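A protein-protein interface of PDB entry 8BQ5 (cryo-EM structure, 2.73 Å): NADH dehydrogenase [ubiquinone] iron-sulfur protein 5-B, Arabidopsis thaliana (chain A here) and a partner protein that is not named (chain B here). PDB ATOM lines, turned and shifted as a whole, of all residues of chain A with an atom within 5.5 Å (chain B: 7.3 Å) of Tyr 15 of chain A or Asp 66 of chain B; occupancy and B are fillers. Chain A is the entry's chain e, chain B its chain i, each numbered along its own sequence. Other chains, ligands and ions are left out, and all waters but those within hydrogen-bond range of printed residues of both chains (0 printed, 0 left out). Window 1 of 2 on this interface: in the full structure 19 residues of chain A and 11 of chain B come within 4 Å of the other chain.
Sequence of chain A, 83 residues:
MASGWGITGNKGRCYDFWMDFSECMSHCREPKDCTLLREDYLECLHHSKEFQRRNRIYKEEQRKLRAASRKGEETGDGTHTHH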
ATOM      1  N   ALA A   2     -19.113 -12.956   7.111  1.00  0.00           N
ATOM      2  CA  ALA A   2     -17.789 -12.896   6.499  1.00  0.00           C
ATOM      3  C   ALA A   2     -17.314 -11.460   6.287  1.00  0.00           C
ATOM      4  O   ALA A   2     -16.120 -11.216   6.137  1.00  0.00           O
ATOM      5  CB  ALA A   2     -17.786 -13.649   5.176  1.00  0.00           C
ATOM      6  N   SER A   3     -18.250 -10.507   6.269  1.00  0.00           N
ATOM      7  CA  SER A   3     -17.874  -9.122   5.995  1.00  0.00           C
ATOM      8  C   SER A   3     -17.377  -8.408   7.246  1.00  0.00           C
ATOM      9  O   SER A   3     -16.586  -7.465   7.146  1.00  0.00           O
ATOM     10  CB  SER A   3     -19.052  -8.364   5.382  1.00  0.00           C
ATOM     11  OG  SER A   3     -19.943  -7.897   6.378  1.00  0.00           O
ATOM     12  N   GLY A   4     -17.830  -8.833   8.423  1.00  0.00           N
ATOM     13  CA  GLY A   4     -17.390  -8.249   9.669  1.00  0.00           C
ATOM     14  C   GLY A   4     -18.203  -7.074  10.165  1.00  0.00           C
ATOM     15  O   GLY A   4     -17.980  -6.625  11.295  1.00  0.00           O
ATOM     16  N   LYS A  11     -18.129  -5.657  15.631  1.00  0.00           N
ATOM     17  CA  LYS A  11     -17.662  -6.768  14.813  1.00  0.00           C
ATOM     18  C   LYS A  11     -18.710  -7.872  14.787  1.00  0.00           C
ATOM     19  O   LYS A  11     -19.305  -8.202  15.816  1.00  0.00           O
ATOM     20  CB  LYS A  11     -16.336  -7.310  15.351  1.00  0.00           C
ATOM     21  CG  LYS A  11     -15.956  -8.666  14.771  1.00  0.00           C
ATOM     22  CD  LYS A  11     -14.604  -9.165  15.257  1.00  0.00           C
ATOM     23  CE  LYS A  11     -13.594  -8.044  15.377  1.00  0.00           C
ATOM     24  NZ  LYS A  11     -12.536  -8.381  16.365  1.00  0.00           N
ATOM     25  N   GLY A  12     -18.935  -8.441  13.605  1.00  0.00           N
ATOM     26  CA  GLY A  12     -19.901  -9.510  13.449  1.00  0.00           C
ATOM     27  C   GLY A  12     -19.599 -10.714  14.318  1.00  0.00           C
ATOM     28  O   GLY A  12     -18.444 -10.950  14.684  1.00  0.00           O
ATOM     29  N   ARG A  13     -20.638 -11.484  14.653  1.00  0.00           N
ATOM     30  CA  ARG A  13     -20.480 -12.586  15.598  1.00  0.00           C
ATOM     31  C   ARG A  13     -19.524 -13.647  15.070  1.00  0.00           C
ATOM     32  O   ARG A  13     -18.693 -14.173  15.819  1.00  0.00           O
ATOM     33  CB  ARG A  13     -21.844 -13.202  15.912  1.00  0.00           C
ATOM     34  CG  ARG A  13     -21.779 -14.590  16.534  1.00  0.00           C
ATOM     35  CD  ARG A  13     -23.166 -15.124  16.842  1.00  0.00           C
ATOM     36  NE  ARG A  13     -23.653 -16.030  15.808  1.00  0.00           N
ATOM     37  CZ  ARG A  13     -24.620 -15.732  14.952  1.00  0.00           C
ATOM     38  NH1 ARG A  13     -25.216 -14.552  14.969  1.00  0.00           N
ATOM     39  NH2 ARG A  13     -24.995 -16.638  14.054  1.00  0.00           N
ATOM     40  N   CYS A  14     -19.618 -13.968  13.783  1.00  0.00           N
ATOM     41  CA  CYS A  14     -18.877 -15.071  13.192  1.00  0.00           C
ATOM     42  C   CYS A  14     -17.664 -14.616  12.394  1.00  0.00           C
ATOM     43  O   CYS A  14     -17.111 -15.405  11.625  1.00  0.00           O
ATOM     44  CB  CYS A  14     -19.807 -15.897  12.305  1.00  0.00           C
ATOM     45  SG  CYS A  14     -21.199 -16.596  13.202  1.00  0.00           S
ATOM     46  N   TYR A  15     -17.235 -13.365  12.564  1.00  0.00           N
ATOM     47  CA  TYR A  15     -16.180 -12.828  11.712  1.00  0.00           C
ATOM     48  C   TYR A  15     -14.823 -13.437  12.039  1.00  0.00           C
ATOM     49  O   TYR A  15     -14.026 -13.699  11.134  1.00  0.00           O
ATOM     50  CB  TYR A  15     -16.125 -11.309  11.837  1.00  0.00           C
ATOM     51  CG  TYR A  15     -15.027 -10.677  11.020  1.00  0.00           C
ATOM     52  CD1 TYR A  15     -15.050 -10.734   9.633  1.00  0.00           C
ATOM     53  CD2 TYR A  15     -13.963 -10.034  11.633  1.00  0.00           C
ATOM     54  CE1 TYR A  15     -14.052 -10.155   8.880  1.00  0.00           C
ATOM     55  CE2 TYR A  15     -12.960  -9.454  10.890  1.00  0.00           C
ATOM     56  CZ  TYR A  15     -13.009  -9.517   9.514  1.00  0.00           C
ATOM     57  OH  TYR A  15     -12.009  -8.942   8.767  1.00  0.00           O
ATOM     58  N   ASP A  16     -14.529 -13.651  13.324  1.00  0.00           N
ATOM     59  CA  ASP A  16     -13.240 -14.225  13.696  1.00  0.00           C
ATOM     60  C   ASP A  16     -13.092 -15.647  13.172  1.00  0.00           C
ATOM     61  O   ASP A  16     -12.022 -16.029  12.688  1.00  0.00           O
ATOM     62  CB  ASP A  16     -13.069 -14.190  15.211  1.00  0.00           C
ATOM     63  CG  ASP A  16     -12.710 -12.814  15.719  1.00  0.00           C
ATOM     64  OD1 ASP A  16     -12.182 -12.009  14.926  1.00  0.00           O
ATOM     65  OD2 ASP A  16     -12.965 -12.535  16.908  1.00  0.00           O
ATOM     66  N   PHE A  17     -14.155 -16.447  13.258  1.00  0.00           N
ATOM     67  CA  PHE A  17     -14.119 -17.785  12.683  1.00  0.00           C
ATOM     68  C   PHE A  17     -13.870 -17.720  11.183  1.00  0.00           C
ATOM     69  O   PHE A  17     -13.071 -18.492  10.635  1.00  0.00           O
ATOM     70  CB  PHE A  17     -15.428 -18.514  12.973  1.00  0.00           C
ATOM     71  CG  PHE A  17     -15.559 -18.981  14.387  1.00  0.00           C
ATOM     72  CD1 PHE A  17     -14.709 -19.949  14.886  1.00  0.00           C
ATOM     73  CD2 PHE A  17     -16.536 -18.462  15.217  1.00  0.00           C
ATOM     74  CE1 PHE A  17     -14.825 -20.386  16.184  1.00  0.00           C
ATOM     75  CE2 PHE A  17     -16.657 -18.899  16.517  1.00  0.00           C
ATOM     76  CZ  PHE A  17     -15.799 -19.860  17.002  1.00  0.00           C
ATOM     77  N   TRP A  18     -14.551 -16.795  10.503  1.00  0.00           N
ATOM     78  CA  TRP A  18     -14.361 -16.640   9.068  1.00  0.00           C
ATOM     79  C   TRP A  18     -12.926 -16.277   8.751  1.00  0.00           C
ATOM     80  O   TRP A  18     -12.321 -16.818   7.816  1.00  0.00           O
ATOM     81  CB  TRP A  18     -15.281 -15.559   8.513  1.00  0.00           C
ATOM     82  CG  TRP A  18     -14.831 -15.147   7.159  1.00  0.00           C
ATOM     83  CD1 TRP A  18     -14.255 -13.962   6.801  1.00  0.00           C
ATOM     84  CD2 TRP A  18     -14.866 -15.948   5.980  1.00  0.00           C
ATOM     85  NE1 TRP A  18     -13.954 -13.971   5.462  1.00  0.00           N
ATOM     86  CE2 TRP A  18     -14.320 -15.182   4.936  1.00  0.00           C
ATOM     87  CE3 TRP A  18     -15.321 -17.238   5.705  1.00  0.00           C
ATOM     88  CZ2 TRP A  18     -14.217 -15.665   3.637  1.00  0.00           C
ATOM     89  CZ3 TRP A  18     -15.215 -17.713   4.425  1.00  0.00           C
ATOM     90  CH2 TRP A  18     -14.672 -16.930   3.402  1.00  0.00           C
ATOM     91  N   MET A  19     -12.374 -15.333   9.505  1.00  0.00           N
ATOM     92  CA  MET A  19     -11.009 -14.954   9.229  1.00  0.00           C
ATOM     93  C   MET A  19     -10.106 -16.157   9.414  1.00  0.00           C
ATOM     94  O   MET A  19      -9.462 -16.573   8.449  1.00  0.00           O
ATOM     95  CB  MET A  19     -10.603 -13.748  10.076  1.00  0.00           C
ATOM     96  CG  MET A  19     -11.155 -12.448   9.485  1.00  0.00           C
ATOM     97  SD  MET A  19     -10.938 -12.346   7.688  1.00  0.00           S
ATOM     98  CE  MET A  19      -9.730 -11.033   7.552  1.00  0.00           C
ATOM     99  N   ASP A  20     -10.156 -16.824  10.573  1.00  0.00           N
ATOM    100  CA  ASP A  20      -9.268 -17.965  10.809  1.00  0.00           C
ATOM    101  C   ASP A  20      -9.373 -18.997   9.688  1.00  0.00           C
ATOM    102  O   ASP A  20      -8.356 -19.523   9.216  1.00  0.00           O
ATOM    103  CB  ASP A  20      -9.574 -18.596  12.166  1.00  0.00           C
ATOM    104  CG  ASP A  20      -9.351 -17.633  13.307  1.00  0.00           C
ATOM    105  OD1 ASP A  20      -9.553 -16.420  13.108  1.00  0.00           O
ATOM    106  OD2 ASP A  20      -8.963 -18.081  14.403  1.00  0.00           O
ATOM    107  N   ALA B  61      -7.494 -10.837  -1.226  1.00  0.00           N
ATOM    108  CA  ALA B  61      -7.633  -9.397  -1.044  1.00  0.00           C
ATOM    109  C   ALA B  61      -8.189  -9.047   0.331  1.00  0.00           C
ATOM    110  O   ALA B  61      -7.718  -8.099   0.970  1.00  0.00           O
ATOM    111  CB  ALA B  61      -8.513  -8.821  -2.149  1.00  0.00           C
ATOM    112  N   GLN B  62      -9.194  -9.792   0.807  1.00  0.00           N
ATOM    113  CA  GLN B  62      -9.785  -9.467   2.105  1.00  0.00           C
ATOM    114  C   GLN B  62      -8.767  -9.636   3.226  1.00  0.00           C
ATOM    115  O   GLN B  62      -8.748  -8.851   4.180  1.00  0.00           O
ATOM    116  CB  GLN B  62     -11.025 -10.327   2.371  1.00  0.00           C
ATOM    117  CG  GLN B  62     -11.540 -10.231   3.811  1.00  0.00           C
ATOM    118  CD  GLN B  62     -12.911 -10.855   4.012  1.00  0.00           C
ATOM    119  OE1 GLN B  62     -13.249 -11.860   3.391  1.00  0.00           O
ATOM    120  NE2 GLN B  62     -13.707 -10.257   4.892  1.00  0.00           N
ATOM    121  N   LEU B  63      -7.903 -10.645   3.113  1.00  0.00           N
ATOM    122  CA  LEU B  63      -6.871 -10.879   4.115  1.00  0.00           C
ATOM    123  C   LEU B  63      -5.883  -9.726   4.224  1.00  0.00           C
ATOM    124  O   LEU B  63      -5.262  -9.561   5.279  1.00  0.00           O
ATOM    125  CB  LEU B  63      -6.129 -12.175   3.798  1.00  0.00           C
ATOM    126  CG  LEU B  63      -6.618 -13.346   4.642  1.00  0.00           C
ATOM    127  CD1 LEU B  63      -6.321 -14.672   3.981  1.00  0.00           C
ATOM    128  CD2 LEU B  63      -5.962 -13.254   5.997  1.00  0.00           C
ATOM    129  N   ARG B  64      -5.715  -8.931   3.168  1.00  0.00           N
ATOM    130  CA  ARG B  64      -4.839  -7.768   3.237  1.00  0.00           C
ATOM    131  C   ARG B  64      -5.587  -6.457   3.428  1.00  0.00           C
ATOM    132  O   ARG B  64      -5.008  -5.509   3.965  1.00  0.00           O
ATOM    133  CB  ARG B  64      -3.971  -7.669   1.974  1.00  0.00           C
ATOM    134  CG  ARG B  64      -3.562  -9.008   1.383  1.00  0.00           C
ATOM    135  CD  ARG B  64      -2.214  -8.930   0.669  1.00  0.00           C
ATOM    136  NE  ARG B  64      -2.304  -8.361  -0.671  1.00  0.00           N
ATOM    137  CZ  ARG B  64      -1.813  -7.180  -1.022  1.00  0.00           C
ATOM    138  NH1 ARG B  64      -1.205  -6.397  -0.145  1.00  0.00           N
ATOM    139  NH2 ARG B  64      -1.927  -6.778  -2.283  1.00  0.00           N
ATOM    140  N   TRP B  65      -6.854  -6.380   3.015  1.00  0.00           N
ATOM    141  CA  TRP B  65      -7.596  -5.129   3.127  1.00  0.00           C
ATOM    142  C   TRP B  65      -8.210  -4.962   4.512  1.00  0.00           C
ATOM    143  O   TRP B  65      -8.057  -3.910   5.139  1.00  0.00           O
ATOM    144  CB  TRP B  65      -8.679  -5.064   2.049  1.00  0.00           C
ATOM    145  CG  TRP B  65      -9.611  -3.901   2.199  1.00  0.00           C
ATOM    146  CD1 TRP B  65     -10.951  -3.950   2.445  1.00  0.00           C
ATOM    147  CD2 TRP B  65      -9.268  -2.512   2.124  1.00  0.00           C
ATOM    148  NE1 TRP B  65     -11.466  -2.680   2.520  1.00  0.00           N
ATOM    149  CE2 TRP B  65     -10.453  -1.779   2.329  1.00  0.00           C
ATOM    150  CE3 TRP B  65      -8.075  -1.817   1.909  1.00  0.00           C
ATOM    151  CZ2 TRP B  65     -10.478  -0.389   2.321  1.00  0.00           C
ATOM    152  CZ3 TRP B  65      -8.104  -0.436   1.901  1.00  0.00           C
ATOM    153  CH2 TRP B  65      -9.297   0.263   2.105  1.00  0.00           C
ATOM    154  N   ASP B  66      -8.895  -5.992   5.003  1.00  0.00           N
ATOM    155  CA  ASP B  66      -9.624  -5.890   6.267  1.00  0.00           C
ATOM    156  C   ASP B  66      -8.782  -5.432   7.454  1.00  0.00           C
ATOM    157  O   ASP B  66      -9.302  -4.652   8.271  1.00  0.00           O
ATOM    158  CB  ASP B  66     -10.299  -7.233   6.579  1.00  0.00           C
ATOM    159  CG  ASP B  66     -11.695  -7.333   5.994  1.00  0.00           C
ATOM    160  OD1 ASP B  66     -12.060  -6.469   5.171  1.00  0.00           O
ATOM    161  OD2 ASP B  66     -12.430  -8.270   6.365  1.00  0.00           O
ATOM    162  N   PRO B  67      -7.528  -5.866   7.639  1.00  0.00           N
ATOM    163  CA  PRO B  67      -6.749  -5.339   8.773  1.00  0.00           C
ATOM    164  C   PRO B  67      -6.537  -3.837   8.723  1.00  0.00           C
ATOM    165  O   PRO B  67      -6.230  -3.233   9.757  1.00  0.00           O
ATOM    166  CB  PRO B  67      -5.418  -6.095   8.670  1.00  0.00           C
ATOM    167  CG  PRO B  67      -5.735  -7.324   7.936  1.00  0.00           C
ATOM    168  CD  PRO B  67      -6.839  -6.993   6.985  1.00  0.00           C
ATOM    169  N   GLN B  68      -6.685  -3.213   7.554  1.00  0.00           N
ATOM    170  CA  GLN B  68      -6.533  -1.767   7.465  1.00  0.00           C
ATOM    171  C   GLN B  68      -7.766  -1.018   7.960  1.00  0.00           C
ATOM    172  O   GLN B  68      -7.688   0.196   8.177  1.00  0.00           O
ATOM    173  CB  GLN B  68      -6.221  -1.358   6.025  1.00  0.00           C
ATOM    174  CG  GLN B  68      -4.923  -1.929   5.485  1.00  0.00           C
ATOM    175  CD  GLN B  68      -4.673  -1.539   4.044  1.00  0.00           C
ATOM    176  OE1 GLN B  68      -4.693  -0.360   3.696  1.00  0.00           O
ATOM    177  NE2 GLN B  68      -4.442  -2.531   3.194  1.00  0.00           N
ATOM    178  N   ILE B  69      -8.893  -1.701   8.143  1.00  0.00           N
ATOM    179  CA  ILE B  69     -10.108  -1.074   8.648  1.00  0.00           C
ATOM    180  C   ILE B  69     -10.555  -1.707   9.965  1.00  0.00           C
ATOM    181  O   ILE B  69     -11.690  -1.510  10.390  1.00  0.00           O
ATOM    182  CB  ILE B  69     -11.242  -1.116   7.609  1.00  0.00           C
ATOM    183  CG1 ILE B  69     -11.423  -2.531   7.058  1.00  0.00           C
ATOM    184  CG2 ILE B  69     -10.989  -0.116   6.494  1.00  0.00           C
ATOM    185  CD1 ILE B  69     -12.781  -2.775   6.443  1.00  0.00           C
ATOM    186  N   SER B  70      -9.672  -2.462  10.623  1.00  0.00           N
ATOM    187  CA  SER B  70     -10.056  -3.171  11.838  1.00  0.00           C
ATOM    188  C   SER B  70     -10.409  -2.229  12.982  1.00  0.00           C
ATOM    189  O   SER B  70     -11.066  -2.656  13.936  1.00  0.00           O
ATOM    190  CB  SER B  70      -8.936  -4.121  12.273  1.00  0.00           C
ATOM    191  OG  SER B  70      -7.674  -3.481  12.237  1.00  0.00           O
ATOM    192  N   GLN B  71      -9.996  -0.966  12.907  1.00  0.00           N
ATOM    193  CA  GLN B  71     -10.284   0.022  13.937  1.00  0.00           C
ATOM    194  C   GLN B  71     -11.414   0.964  13.546  1.00  0.00           C
ATOM    195  O   GLN B  71     -11.665   1.945  14.253  1.00  0.00           O
ATOM    196  CB  GLN B  71      -9.025   0.827  14.255  1.00  0.00           C
ATOM    197  CG  GLN B  71      -7.756   0.000  14.254  1.00  0.00           C
ATOM    198  CD  GLN B  71      -7.302  -0.366  15.647  1.00  0.00           C
ATOM    199  OE1 GLN B  71      -7.226   0.486  16.531  1.00  0.00           O
ATOM    200  NE2 GLN B  71      -6.994  -1.640  15.853  1.00  0.00           N
ATOM    201  N   ARG B  75     -17.205  -2.072  13.010  1.00  0.00           N
ATOM    202  CA  ARG B  75     -16.691  -3.432  12.900  1.00  0.00           C
ATOM    203  C   ARG B  75     -15.665  -3.751  13.984  1.00  0.00           C
ATOM    204  O   ARG B  75     -14.818  -4.628  13.783  1.00  0.00           O
ATOM    205  CB  ARG B  75     -16.073  -3.671  11.520  1.00  0.00           C
ATOM    206  CG  ARG B  75     -14.868  -2.801  11.217  1.00  0.00           C
ATOM    207  CD  ARG B  75     -14.510  -2.887   9.751  1.00  0.00           C
ATOM    208  NE  ARG B  75     -13.932  -4.180   9.413  1.00  0.00           N
ATOM    209  CZ  ARG B  75     -14.561  -5.122   8.725  1.00  0.00           C
ATOM    210  NH1 ARG B  75     -15.805  -4.957   8.307  1.00  0.00           N
ATOM    211  NH2 ARG B  75     -13.928  -6.258   8.452  1.00  0.00           N
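NE2 of Gln 62 of chain B is in hydrogen-bond range of O of Ala 2 of chain A (2.9 Å).
The guanidinium group (NH1) of Arg 75 of chain B sits at hydrogen-bond distance from the backbone carbonyl oxygen (O) of Ser 3 of chain A (2.9 Å).
OH of Tyr 15 of chain A lies within hydrogen-bond range of OD2 of Asp 66 of chain B (2.5 Å).
The side-chain hydroxyl (OH) of Tyr 15 of chain A sits at hydrogen-bond distance from the guanidinium group (NH2) of Arg 75 of chain B (3.3 Å).
The side-chain amide oxygen (OE1) of Gln 62 of chain B lies within hydrogen-bond range of the indole nitrogen (NE1) of Trp 18 of chain A, at 3.0 Å.
Of the 13 printed residues of chain A, 7 touch a printed residue of chain B.
Printed residues of chain A that touch a printed residue of chain B: Ala 2, Ser 3, Gly 4, Lys 11, Tyr 15, Trp 18 and Met 19.
Hydrophobic or aromatic side chains of chain A that line the printed part of chain B: Tyr 15, Trp 18 and Met 19.
Among the printed residues, 8 pairs touch across the chains.
Among the printed residues, no Asp or Glu carboxylate lies within 4 Å of a Lys or Arg side-chain nitrogen of the other chain.
Printed residues of chain B within 4 Å of Tyr 15 of chain A: Asp 66 (2.5 Å) and Arg 75 (3.3 Å).
Of the printed residues of chain B, Ala 2 of chain A touches Gln 62.
Of the printed residues of chain B, Lys 11 of chain A touches Arg 75.
Printed residues of chain B within 4 Å of Gly 4 of chain A: Arg 75 (3.5 Å).
The nearest printed residue of chain B that does not touch Tyr 15 of chain A is Gln 62 of chain B (4.004 Å).
The nearest residue of chain A that does not touch Asp 66 of chain B is Ser 3 of chain A (4.3 Å).
The backbone carbonyl oxygen of Gly 4 of chain A sits at hydrogen-bond distance from the backbone NH of Gly 12 of chain A, at 3.1 Å.
NZ of Lys 11 of chain A lies within salt-bridge range of OD1 of Asp 16 of chain A (3.9 Å).
The side-chain hydroxyl of Tyr 15 of chain A sits close to the side-chain sulfur of Met 19 of chain A, 3.7 Å away.
The side-chain amide nitrogen (NE2) of Gln 62 of chain B sits at hydrogen-bond distance from the side-chain carboxylate (OD2) of Asp 66 of chain B, 2.8 Å away.
The guanidinium group (NH2) of Arg 75 of chain B lies within salt-bridge range of the side-chain carboxylate (OD2) of Asp 66 of chain B (3.3 Å).
Among the printed residues, merely in contact across the chains: Gly 4 of chain A with Arg 75 of chain B (3.5 Å), Lys 11 of chain A with Arg 75 of chain B (3.5 Å) and Met 19 of chain A with Asp 66 of chain B (3.96 Å).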
